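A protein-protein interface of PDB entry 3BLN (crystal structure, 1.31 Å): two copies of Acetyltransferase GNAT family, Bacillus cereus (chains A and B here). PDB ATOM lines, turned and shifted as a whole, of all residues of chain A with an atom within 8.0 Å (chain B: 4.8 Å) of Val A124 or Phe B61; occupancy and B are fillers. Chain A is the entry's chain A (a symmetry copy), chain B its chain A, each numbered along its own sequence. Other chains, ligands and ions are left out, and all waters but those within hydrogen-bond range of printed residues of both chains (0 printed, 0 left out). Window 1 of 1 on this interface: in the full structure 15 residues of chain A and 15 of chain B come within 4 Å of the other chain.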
ATOM      1  N   ASN A  60     -19.570 -14.262  -3.135  1.00  0.00           N
ATOM      2  CA  ASN A  60     -18.554 -13.271  -2.804  1.00  0.00           C
ATOM      3  C   ASN A  60     -18.692 -11.980  -3.628  1.00  0.00           C
ATOM      4  O   ASN A  60     -17.712 -11.330  -3.972  1.00  0.00           O
ATOM      5  CB  ASN A  60     -17.156 -13.923  -2.919  1.00  0.00           C
ATOM      6  CG  ASN A  60     -16.886 -14.462  -4.291  1.00  0.00           C
ATOM      7  OD1 ASN A  60     -17.643 -14.211  -5.221  1.00  0.00           O
ATOM      8  ND2 ASN A  60     -15.798 -15.218  -4.441  1.00  0.00           N
ATOM      9  N   PHE A  61     -19.923 -11.611  -3.971  1.00  0.00           N
ATOM     10  CA  PHE A  61     -20.206 -10.362  -4.682  1.00  0.00           C
ATOM     11  C   PHE A  61     -20.923  -9.447  -3.729  1.00  0.00           C
ATOM     12  O   PHE A  61     -22.146  -9.539  -3.566  1.00  0.00           O
ATOM     13  CB  PHE A  61     -21.044 -10.629  -5.943  1.00  0.00           C
ATOM     14  CG  PHE A  61     -21.323  -9.420  -6.787  1.00  0.00           C
ATOM     15  CD1 PHE A  61     -20.362  -8.911  -7.650  1.00  0.00           C
ATOM     16  CD2 PHE A  61     -22.569  -8.825  -6.779  1.00  0.00           C
ATOM     17  CE1 PHE A  61     -20.641  -7.800  -8.457  1.00  0.00           C
ATOM     18  CE2 PHE A  61     -22.857  -7.742  -7.578  1.00  0.00           C
ATOM     19  CZ  PHE A  61     -21.888  -7.212  -8.416  1.00  0.00           C
ATOM     20  N   PHE A  62     -20.154  -8.601  -3.032  1.00  0.00           N
ATOM     21  CA  PHE A  62     -20.752  -7.760  -1.972  1.00  0.00           C
ATOM     22  C   PHE A  62     -21.608  -8.610  -1.001  1.00  0.00           C
ATOM     23  O   PHE A  62     -22.691  -8.233  -0.588  1.00  0.00           O
ATOM     24  CB  PHE A  62     -21.537  -6.598  -2.595  1.00  0.00           C
ATOM     25  CG  PHE A  62     -20.706  -5.700  -3.473  1.00  0.00           C
ATOM     26  CD1 PHE A  62     -19.969  -4.669  -2.906  1.00  0.00           C
ATOM     27  CD2 PHE A  62     -20.692  -5.852  -4.846  1.00  0.00           C
ATOM     28  CE1 PHE A  62     -19.227  -3.849  -3.685  1.00  0.00           C
ATOM     29  CE2 PHE A  62     -19.934  -5.037  -5.641  1.00  0.00           C
ATOM     30  CZ  PHE A  62     -19.194  -4.013  -5.044  1.00  0.00           C
ATOM     31  N   PHE A  66     -23.634 -14.553  -6.681  1.00  0.00           N
ATOM     32  CA  PHE A  66     -23.451 -14.148  -8.040  1.00  0.00           C
ATOM     33  C   PHE A  66     -23.347 -15.387  -8.917  1.00  0.00           C
ATOM     34  O   PHE A  66     -22.560 -16.293  -8.644  1.00  0.00           O
ATOM     35  CB  PHE A  66     -22.191 -13.263  -8.169  1.00  0.00           C
ATOM     36  CG  PHE A  66     -22.022 -12.605  -9.512  1.00  0.00           C
ATOM     37  CD1 PHE A  66     -21.587 -13.322 -10.597  1.00  0.00           C
ATOM     38  CD2 PHE A  66     -22.325 -11.273  -9.698  1.00  0.00           C
ATOM     39  CE1 PHE A  66     -21.439 -12.726 -11.845  1.00  0.00           C
ATOM     40  CE2 PHE A  66     -22.179 -10.675 -10.939  1.00  0.00           C
ATOM     41  CZ  PHE A  66     -21.719 -11.396 -12.006  1.00  0.00           C
ATOM     42  N   SER A 101     -24.446 -11.178 -14.449  1.00  0.00           N
ATOM     43  CA  SER A 101     -24.152 -10.189 -15.457  1.00  0.00           C
ATOM     44  C   SER A 101     -24.082 -10.809 -16.820  1.00  0.00           C
ATOM     45  O   SER A 101     -23.946 -12.025 -16.953  1.00  0.00           O
ATOM     46  CB  SER A 101     -22.824  -9.488 -15.138  1.00  0.00           C
ATOM     47  OG  SER A 101     -21.682 -10.299 -15.404  1.00  0.00           O
ATOM     48  N   THR A 102     -24.116  -9.953 -17.843  1.00  0.00           N
ATOM     49  CA  THR A 102     -23.771 -10.362 -19.192  1.00  0.00           C
ATOM     50  C   THR A 102     -23.288  -9.152 -19.959  1.00  0.00           C
ATOM     51  O   THR A 102     -23.493  -8.014 -19.529  1.00  0.00           O
ATOM     52  CB  THR A 102     -24.958 -11.060 -19.924  1.00  0.00           C
ATOM     53  OG1 THR A 102     -24.466 -11.660 -21.130  1.00  0.00           O
ATOM     54  CG2 THR A 102     -26.076 -10.078 -20.262  1.00  0.00           C
ATOM     55  N   ASN A 103     -22.635  -9.363 -21.091  1.00  0.00           N
ATOM     56  CA  ASN A 103     -22.186  -8.216 -21.883  1.00  0.00           C
ATOM     57  C   ASN A 103     -23.345  -7.421 -22.412  1.00  0.00           C
ATOM     58  O   ASN A 103     -24.413  -7.984 -22.740  1.00  0.00           O
ATOM     59  CB  ASN A 103     -21.356  -8.677 -23.072  1.00  0.00           C
ATOM     60  CG  ASN A 103     -20.023  -9.229 -22.702  1.00  0.00           C
ATOM     61  OD1 ASN A 103     -19.838 -10.450 -22.702  1.00  0.00           O
ATOM     62  ND2 ASN A 103     -19.061  -8.349 -22.417  1.00  0.00           N
ATOM     63  N   GLU A 104     -23.126  -6.111 -22.576  1.00  0.00           N
ATOM     64  CA  GLU A 104     -24.129  -5.260 -23.230  1.00  0.00           C
ATOM     65  C   GLU A 104     -24.447  -5.733 -24.660  1.00  0.00           C
ATOM     66  O   GLU A 104     -25.576  -5.568 -25.133  1.00  0.00           O
ATOM     67  CB  GLU A 104     -23.658  -3.807 -23.225  1.00  0.00           C
ATOM     68  CG  GLU A 104     -24.562  -2.788 -23.936  1.00  0.00           C
ATOM     69  CD  GLU A 104     -26.002  -2.662 -23.467  1.00  0.00           C
ATOM     70  OE1 GLU A 104     -26.413  -3.198 -22.424  1.00  0.00           O
ATOM     71  OE2 GLU A 104     -26.758  -1.957 -24.210  1.00  0.00           O
ATOM     72  N   SER A 121     -29.320  -3.736 -13.106  1.00  0.00           N
ATOM     73  CA  SER A 121     -28.925  -3.304 -11.756  1.00  0.00           C
ATOM     74  C   SER A 121     -27.497  -2.758 -11.685  1.00  0.00           C
ATOM     75  O   SER A 121     -26.823  -2.885 -10.687  1.00  0.00           O
ATOM     76  CB  SER A 121     -29.058  -4.525 -10.856  1.00  0.00           C
ATOM     77  OG  SER A 121     -28.896  -4.223  -9.457  1.00  0.00           O
ATOM     78  N   GLY A 122     -27.035  -2.214 -12.801  1.00  0.00           N
ATOM     79  CA  GLY A 122     -25.737  -1.580 -12.864  1.00  0.00           C
ATOM     80  C   GLY A 122     -24.920  -2.015 -14.067  1.00  0.00           C
ATOM     81  O   GLY A 122     -25.423  -2.635 -14.999  1.00  0.00           O
ATOM     82  N   ILE A 123     -23.656  -1.634 -14.015  1.00  0.00           N
ATOM     83  CA  ILE A 123     -22.748  -1.791 -15.147  1.00  0.00           C
ATOM     84  C   ILE A 123     -21.334  -1.785 -14.606  1.00  0.00           C
ATOM     85  O   ILE A 123     -21.030  -1.055 -13.667  1.00  0.00           O
ATOM     86  CB  ILE A 123     -22.977  -0.680 -16.205  1.00  0.00           C
ATOM     87  CG1 ILE A 123     -22.073  -0.858 -17.410  1.00  0.00           C
ATOM     88  CG2 ILE A 123     -22.868   0.688 -15.598  1.00  0.00           C
ATOM     89  CD1 ILE A 123     -22.483   0.018 -18.570  1.00  0.00           C
ATOM     90  N   VAL A 124     -20.462  -2.605 -15.230  1.00  0.00           N
ATOM     91  CA  VAL A 124     -19.017  -2.549 -14.932  1.00  0.00           C
ATOM     92  C   VAL A 124     -18.314  -2.352 -16.253  1.00  0.00           C
ATOM     93  O   VAL A 124     -18.388  -3.200 -17.154  1.00  0.00           O
ATOM     94  CB  VAL A 124     -18.503  -3.770 -14.201  1.00  0.00           C
ATOM     95  CG1 VAL A 124     -17.006  -3.565 -13.840  1.00  0.00           C
ATOM     96  CG2 VAL A 124     -19.320  -4.039 -12.949  1.00  0.00           C
ATOM     97  N   GLU A 125     -17.670  -1.194 -16.368  1.00  0.00           N
ATOM     98  CA  GLU A 125     -16.873  -0.830 -17.522  1.00  0.00           C
ATOM     99  C   GLU A 125     -15.410  -1.215 -17.377  1.00  0.00           C
ATOM    100  O   GLU A 125     -14.985  -1.612 -16.308  1.00  0.00           O
ATOM    101  CB  GLU A 125     -16.972   0.681 -17.737  1.00  0.00           C
ATOM    102  CG  GLU A 125     -18.409   1.153 -17.998  1.00  0.00           C
ATOM    103  CD  GLU A 125     -18.635   2.608 -17.823  1.00  0.00           C
ATOM    104  OE1 GLU A 125     -17.805   3.334 -17.254  1.00  0.00           O
ATOM    105  OE2 GLU A 125     -19.719   3.044 -18.279  1.00  0.00           O
ATOM    106  N   ASN A 126     -14.642  -1.098 -18.465  1.00  0.00           N
ATOM    107  CA  ASN A 126     -13.210  -1.398 -18.475  1.00  0.00           C
ATOM    108  C   ASN A 126     -12.854  -2.861 -18.267  1.00  0.00           C
ATOM    109  O   ASN A 126     -11.775  -3.192 -17.840  1.00  0.00           O
ATOM    110  CB  ASN A 126     -12.472  -0.473 -17.487  1.00  0.00           C
ATOM    111  CG  ASN A 126     -12.627   0.987 -17.860  1.00  0.00           C
ATOM    112  OD1 ASN A 126     -13.309   1.784 -17.142  1.00  0.00           O
ATOM    113  ND2 ASN A 126     -12.045   1.357 -18.965  1.00  0.00           N
ATOM    114  N   LEU A 127     -13.774  -3.725 -18.675  1.00  0.00           N
ATOM    115  CA  LEU A 127     -13.578  -5.152 -18.759  1.00  0.00           C
ATOM    116  C   LEU A 127     -13.397  -5.469 -20.241  1.00  0.00           C
ATOM    117  O   LEU A 127     -12.396  -5.069 -20.800  1.00  0.00           O
ATOM    118  CB  LEU A 127     -14.716  -5.912 -18.065  1.00  0.00           C
ATOM    119  CG  LEU A 127     -14.724  -5.703 -16.540  1.00  0.00           C
ATOM    120  CD1 LEU A 127     -16.017  -6.253 -15.947  1.00  0.00           C
ATOM    121  CD2 LEU A 127     -13.508  -6.341 -15.855  1.00  0.00           C
ATOM    122  N   ASP A 128     -14.329  -6.149 -20.907  1.00  0.00           N
ATOM    123  CA  ASP A 128     -14.135  -6.430 -22.332  1.00  0.00           C
ATOM    124  C   ASP A 128     -14.178  -5.089 -23.091  1.00  0.00           C
ATOM    125  O   ASP A 128     -15.046  -4.255 -22.866  1.00  0.00           O
ATOM    126  CB  ASP A 128     -15.217  -7.379 -22.870  1.00  0.00           C
ATOM    127  CG  ASP A 128     -15.242  -8.734 -22.158  1.00  0.00           C
ATOM    128  OD1 ASP A 128     -14.180  -9.255 -21.774  1.00  0.00           O
ATOM    129  OD2 ASP A 128     -16.317  -9.344 -22.008  1.00  0.00           O
ATOM    130  N   ASP A 131     -17.411  -3.233 -24.409  1.00  0.00           N
ATOM    131  CA  ASP A 131     -18.560  -4.104 -24.234  1.00  0.00           C
ATOM    132  C   ASP A 131     -18.716  -4.397 -22.753  1.00  0.00           C
ATOM    133  O   ASP A 131     -18.345  -5.475 -22.281  1.00  0.00           O
ATOM    134  CB  ASP A 131     -18.369  -5.375 -25.053  1.00  0.00           C
ATOM    135  CG  ASP A 131     -19.633  -6.183 -25.215  1.00  0.00           C
ATOM    136  OD1 ASP A 131     -20.705  -5.790 -24.699  1.00  0.00           O
ATOM    137  OD2 ASP A 131     -19.546  -7.267 -25.845  1.00  0.00           O
ATOM    138  N   PRO A 132     -19.273  -3.438 -22.018  1.00  0.00           N
ATOM    139  CA  PRO A 132     -19.344  -3.586 -20.565  1.00  0.00           C
ATOM    140  C   PRO A 132     -20.226  -4.711 -20.086  1.00  0.00           C
ATOM    141  O   PRO A 132     -21.078  -5.223 -20.809  1.00  0.00           O
ATOM    142  CB  PRO A 132     -19.910  -2.257 -20.071  1.00  0.00           C
ATOM    143  CG  PRO A 132     -20.118  -1.440 -21.210  1.00  0.00           C
ATOM    144  CD  PRO A 132     -19.781  -2.140 -22.464  1.00  0.00           C
ATOM    145  N   GLU A 133     -19.995  -5.114 -18.835  1.00  0.00           N
ATOM    146  CA  GLU A 133     -20.854  -6.061 -18.170  1.00  0.00           C
ATOM    147  C   GLU A 133     -22.047  -5.344 -17.604  1.00  0.00           C
ATOM    148  O   GLU A 133     -21.887  -4.393 -16.822  1.00  0.00           O
ATOM    149  CB  GLU A 133     -20.113  -6.778 -17.021  1.00  0.00           C
ATOM    150  CG  GLU A 133     -19.028  -7.731 -17.493  1.00  0.00           C
ATOM    151  CD  GLU A 133     -19.552  -8.923 -18.213  1.00  0.00           C
ATOM    152  OE1 GLU A 133     -20.615  -9.455 -17.872  1.00  0.00           O
ATOM    153  OE2 GLU A 133     -18.852  -9.425 -19.115  1.00  0.00           O
ATOM    154  N   ILE A 134     -23.230  -5.813 -17.958  1.00  0.00           N
ATOM    155  CA  ILE A 134     -24.463  -5.303 -17.380  1.00  0.00           C
ATOM    156  C   ILE A 134     -24.825  -6.181 -16.220  1.00  0.00           C
ATOM    157  O   ILE A 134     -24.926  -7.395 -16.373  1.00  0.00           O
ATOM    158  CB  ILE A 134     -25.597  -5.280 -18.417  1.00  0.00           C
ATOM    159  CG1 ILE A 134     -25.147  -4.492 -19.657  1.00  0.00           C
ATOM    160  CG2 ILE A 134     -26.892  -4.780 -17.770  1.00  0.00           C
ATOM    161  CD1 ILE A 134     -24.650  -3.030 -19.378  1.00  0.00           C
ATOM    162  N   ILE A 135     -25.002  -5.586 -15.050  1.00  0.00           N
ATOM    163  CA  ILE A 135     -25.368  -6.316 -13.836  1.00  0.00           C
ATOM    164  C   ILE A 135     -26.870  -6.543 -13.817  1.00  0.00           C
ATOM    165  O   ILE A 135     -27.642  -5.632 -14.132  1.00  0.00           O
ATOM    166  CB  ILE A 135     -24.910  -5.557 -12.563  1.00  0.00           C
ATOM    167  CG1 ILE A 135     -23.418  -5.212 -12.570  1.00  0.00           C
ATOM    168  CG2 ILE A 135     -25.312  -6.297 -11.274  1.00  0.00           C
ATOM    169  CD1 ILE A 135     -22.511  -6.430 -12.636  1.00  0.00           C
ATOM    170  N   THR B  59      -8.678 -11.340  -5.964  1.00  0.00           N
ATOM    171  CA  THR B  59      -8.498 -11.341  -7.379  1.00  0.00           C
ATOM    172  C   THR B  59      -9.690 -11.991  -8.058  1.00  0.00           C
ATOM    173  O   THR B  59      -9.583 -12.532  -9.170  1.00  0.00           O
ATOM    174  CB  THR B  59      -7.207 -11.994  -7.784  1.00  0.00           C
ATOM    175  OG1 THR B  59      -7.223 -13.334  -7.279  1.00  0.00           O
ATOM    176  CG2 THR B  59      -6.034 -11.245  -7.243  1.00  0.00           C
ATOM    177  N   ASN B  60     -10.858 -11.849  -7.458  1.00  0.00           N
ATOM    178  CA  ASN B  60     -12.019 -12.588  -7.939  1.00  0.00           C
ATOM    179  C   ASN B  60     -13.146 -11.667  -8.433  1.00  0.00           C
ATOM    180  O   ASN B  60     -14.326 -11.968  -8.297  1.00  0.00           O
ATOM    181  CB  ASN B  60     -12.475 -13.581  -6.845  1.00  0.00           C
ATOM    182  CG  ASN B  60     -12.828 -12.895  -5.560  1.00  0.00           C
ATOM    183  OD1 ASN B  60     -12.915 -11.674  -5.507  1.00  0.00           O
ATOM    184  ND2 ASN B  60     -13.039 -13.672  -4.497  1.00  0.00           N
ATOM    185  N   PHE B  61     -12.785 -10.516  -8.994  1.00  0.00           N
ATOM    186  CA  PHE B  61     -13.750  -9.585  -9.582  1.00  0.00           C
ATOM    187  C   PHE B  61     -13.549  -9.599 -11.071  1.00  0.00           C
ATOM    188  O   PHE B  61     -12.673  -8.899 -11.596  1.00  0.00           O
ATOM    189  CB  PHE B  61     -13.568  -8.172  -9.003  1.00  0.00           C
ATOM    190  CG  PHE B  61     -14.563  -7.156  -9.485  1.00  0.00           C
ATOM    191  CD1 PHE B  61     -15.845  -7.103  -8.956  1.00  0.00           C
ATOM    192  CD2 PHE B  61     -14.204  -6.202 -10.415  1.00  0.00           C
ATOM    193  CE1 PHE B  61     -16.758  -6.132  -9.388  1.00  0.00           C
ATOM    194  CE2 PHE B  61     -15.088  -5.236 -10.836  1.00  0.00           C
ATOM    195  CZ  PHE B  61     -16.381  -5.202 -10.334  1.00  0.00           C
ATOM    196  N   PHE B  62     -14.312 -10.456 -11.762  1.00  0.00           N
ATOM    197  CA  PHE B  62     -14.090 -10.640 -13.213  1.00  0.00           C
ATOM    198  C   PHE B  62     -12.595 -10.906 -13.519  1.00  0.00           C
ATOM    199  O   PHE B  62     -12.023 -10.390 -14.464  1.00  0.00           O
ATOM    200  CB  PHE B  62     -14.654  -9.446 -13.993  1.00  0.00           C
ATOM    201  CG  PHE B  62     -16.128  -9.219 -13.784  1.00  0.00           C
ATOM    202  CD1 PHE B  62     -17.050  -9.929 -14.544  1.00  0.00           C
ATOM    203  CD2 PHE B  62     -16.589  -8.286 -12.877  1.00  0.00           C
ATOM    204  CE1 PHE B  62     -18.376  -9.726 -14.373  1.00  0.00           C
ATOM    205  CE2 PHE B  62     -17.929  -8.085 -12.687  1.00  0.00           C
ATOM    206  CZ  PHE B  62     -18.835  -8.818 -13.457  1.00  0.00           C
ATOM    207  N   ASP B  63     -11.981 -11.722 -12.674  1.00  0.00           N
ATOM    208  CA  ASP B  63     -10.575 -12.157 -12.778  1.00  0.00           C
ATOM    209  C   ASP B  63      -9.560 -11.038 -12.544  1.00  0.00           C
ATOM    210  O   ASP B  63      -8.367 -11.195 -12.832  1.00  0.00           O
ATOM    211  CB  ASP B  63     -10.291 -12.876 -14.103  1.00  0.00           C
ATOM    212  CG  ASP B  63     -11.003 -14.199 -14.200  1.00  0.00           C
ATOM    213  OD1 ASP B  63     -11.097 -14.900 -13.169  1.00  0.00           O
ATOM    214  OD2 ASP B  63     -11.459 -14.518 -15.302  1.00  0.00           O
ATOM    215  N   CYS B  64     -10.023  -9.941 -11.963  1.00  0.00           N
ATOM    216  CA  CYS B  64      -9.185  -8.793 -11.668  1.00  0.00           C
ATOM    217  C   CYS B  64      -9.113  -8.563 -10.161  1.00  0.00           C
ATOM    218  O   CYS B  64      -9.979  -8.962  -9.390  1.00  0.00           O
ATOM    219  CB  CYS B  64      -9.761  -7.540 -12.319  1.00  0.00           C
ATOM    220  SG  CYS B  64      -9.860  -7.624 -14.122  1.00  0.00           S
ATOM    221  N   PHE B  66      -9.615  -6.629  -6.848  1.00  0.00           N
ATOM    222  CA  PHE B  66     -10.554  -5.714  -6.274  1.00  0.00           C
ATOM    223  C   PHE B  66     -10.129  -5.398  -4.847  1.00  0.00           C
ATOM    224  O   PHE B  66      -9.882  -6.298  -4.045  1.00  0.00           O
ATOM    225  CB  PHE B  66     -11.977  -6.313  -6.315  1.00  0.00           C
ATOM    226  CG  PHE B  66     -13.072  -5.353  -5.936  1.00  0.00           C
ATOM    227  CD1 PHE B  66     -13.290  -5.016  -4.625  1.00  0.00           C
ATOM    228  CD2 PHE B  66     -13.870  -4.763  -6.894  1.00  0.00           C
ATOM    229  CE1 PHE B  66     -14.292  -4.121  -4.264  1.00  0.00           C
ATOM    230  CE2 PHE B  66     -14.869  -3.872  -6.540  1.00  0.00           C
ATOM    231  CZ  PHE B  66     -15.091  -3.565  -5.227  1.00  0.00           C
ATOM    232  N   PHE B  99      -9.683  -2.744  -9.528  1.00  0.00           N
ATOM    233  CA  PHE B  99     -10.987  -2.171  -9.280  1.00  0.00           C
ATOM    234  C   PHE B  99     -11.189  -1.999  -7.763  1.00  0.00           C
ATOM    235  O   PHE B  99     -10.535  -2.634  -6.926  1.00  0.00           O
ATOM    236  CB  PHE B  99     -12.097  -3.086  -9.822  1.00  0.00           C
ATOM    237  CG  PHE B  99     -12.165  -3.171 -11.328  1.00  0.00           C
ATOM    238  CD1 PHE B  99     -11.458  -4.120 -12.015  1.00  0.00           C
ATOM    239  CD2 PHE B  99     -12.994  -2.300 -12.018  1.00  0.00           C
ATOM    240  CE1 PHE B  99     -11.618  -4.218 -13.396  1.00  0.00           C
ATOM    241  CE2 PHE B  99     -13.158  -2.394 -13.365  1.00  0.00           C
ATOM    242  CZ  PHE B  99     -12.439  -3.339 -14.069  1.00  0.00           C
ATOM    243  N   SER B 121     -16.109   3.833 -13.093  1.00  0.00           N
ATOM    244  CA  SER B 121     -16.098   2.690 -14.020  1.00  0.00           C
ATOM    245  C   SER B 121     -17.312   1.771 -13.869  1.00  0.00           C
ATOM    246  O   SER B 121     -17.233   0.582 -14.084  1.00  0.00           O
ATOM    247  CB  SER B 121     -14.821   1.913 -13.730  1.00  0.00           C
ATOM    248  OG  SER B 121     -14.558   0.869 -14.687  1.00  0.00           O
ATOM    249  N   GLY B 122     -18.416   2.350 -13.421  1.00  0.00           N
ATOM    250  CA  GLY B 122     -19.665   1.631 -13.308  1.00  0.00           C
ATOM    251  C   GLY B 122     -20.356   1.844 -11.973  1.00  0.00           C
ATOM    252  O   GLY B 122     -20.005   2.729 -11.199  1.00  0.00           O
ATOM    253  N   ILE B 135     -18.274   1.922  -8.909  1.00  0.00           N
ATOM    254  CA  ILE B 135     -17.062   1.173  -9.243  1.00  0.00           C
ATOM    255  C   ILE B 135     -15.983   2.139  -9.702  1.00  0.00           C
ATOM    256  O   ILE B 135     -16.259   3.059 -10.478  1.00  0.00           O
ATOM    257  CB  ILE B 135     -17.342   0.104 -10.332  1.00  0.00           C
ATOM    258  CG1 ILE B 135     -18.491  -0.841  -9.967  1.00  0.00           C
ATOM    259  CG2 ILE B 135     -16.071  -0.675 -10.716  1.00  0.00           C
ATOM    260  CD1 ILE B 135     -18.242  -1.642  -8.699  1.00  0.00           C
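ND2 of Asn A60 sits close to ND2 of Asn B60 (3.2 Å). The backbone NH (N) of Glu A125 is in hydrogen-bond range of the backbone carbonyl oxygen (O) of Ser B121, at 2.9 Å. The side-chain hydroxyl of Ser B121 is in hydrogen-bond range of the side-chain amide oxygen of Asn A126.
The backbone carbonyl oxygen (O) of Phe B62 lies within hydrogen-bond range of the side-chain sulfur (SG) of Cys B64, 3.5 Å away. The backbone NH (N) of Ser B121 sits at hydrogen-bond distance from the backbone carbonyl oxygen (O) of Ile B135 (2.7 Å). The backbone carbonyl oxygen (O) of Gly B122 sits at hydrogen-bond distance from the backbone NH (N) of Ile B135 (3.0 Å). OG of Ser A101 is in hydrogen-bond range of OE1 of Glu A133. The side-chain carboxylate (OE2) of Glu A133 sits at hydrogen-bond distance from the side-chain amide nitrogen (ND2) of Asn A103. N of Val A124 is in hydrogen-bond range of O of Glu A133, at 2.8 Å.
Among the printed residues, pairs that only touch across the chains: Ser A101 with Phe B62 (3.5 Å), Ile A123 with Gly B122 (3.0 Å), Val A124 with Phe B61 (3.9 Å), Val A124 with Ser B121 (3.7 Å), Glu A125 with Phe B99 (3.6 Å), Asn A126 with Phe B99 (3.8 Å), Leu A127 with Phe B62 (3.7 Å), Leu A127 with Phe B99 (3.7 Å) and Glu A133 with Phe B62 (3.8 Å).
Gly A122 touches none of the printed residues of chain B. Val A124 touches just these residues of chain B: Phe B61 (3.9 Å) and Ser B121 (3.7 Å). Of the printed residues of chain B, Asn A126 touches Phe B99 (3.8 Å) and Ser B121 (2.9 Å). Of chain A, only Val A124 comes within 4 Å of Phe B61. Of the printed residues of chain A, Phe B62 touches Ser A101 (3.5 Å), Leu A127 (3.7 Å) and Glu A133 (3.8 Å). The nearest residue of chain B that does not touch Val A124 is Phe B99 (4.1 Å). The nearest residue of chain A that does not touch Phe B61 is Phe A61 (4.3 Å). The nearest printed residue of chain A that does not touch Phe B62 is Phe A66 (4.1 Å).
Of the 11 printed residues of chain B, 6 touch a printed residue of chain A. Along chain A the printed residues that touch a printed residue of chain B span positions 60 to 133. Among the printed residues, 12 pairs touch across the chains.
Asn B60 touches its own counterpart, Asn A60. Positions printed for both chains: 60, 61, 62, 66, 121, 122 and 135. Of the 12 pairs that touch across the chains among the printed residues, 1 has its exchanged pair printed and touching as well.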
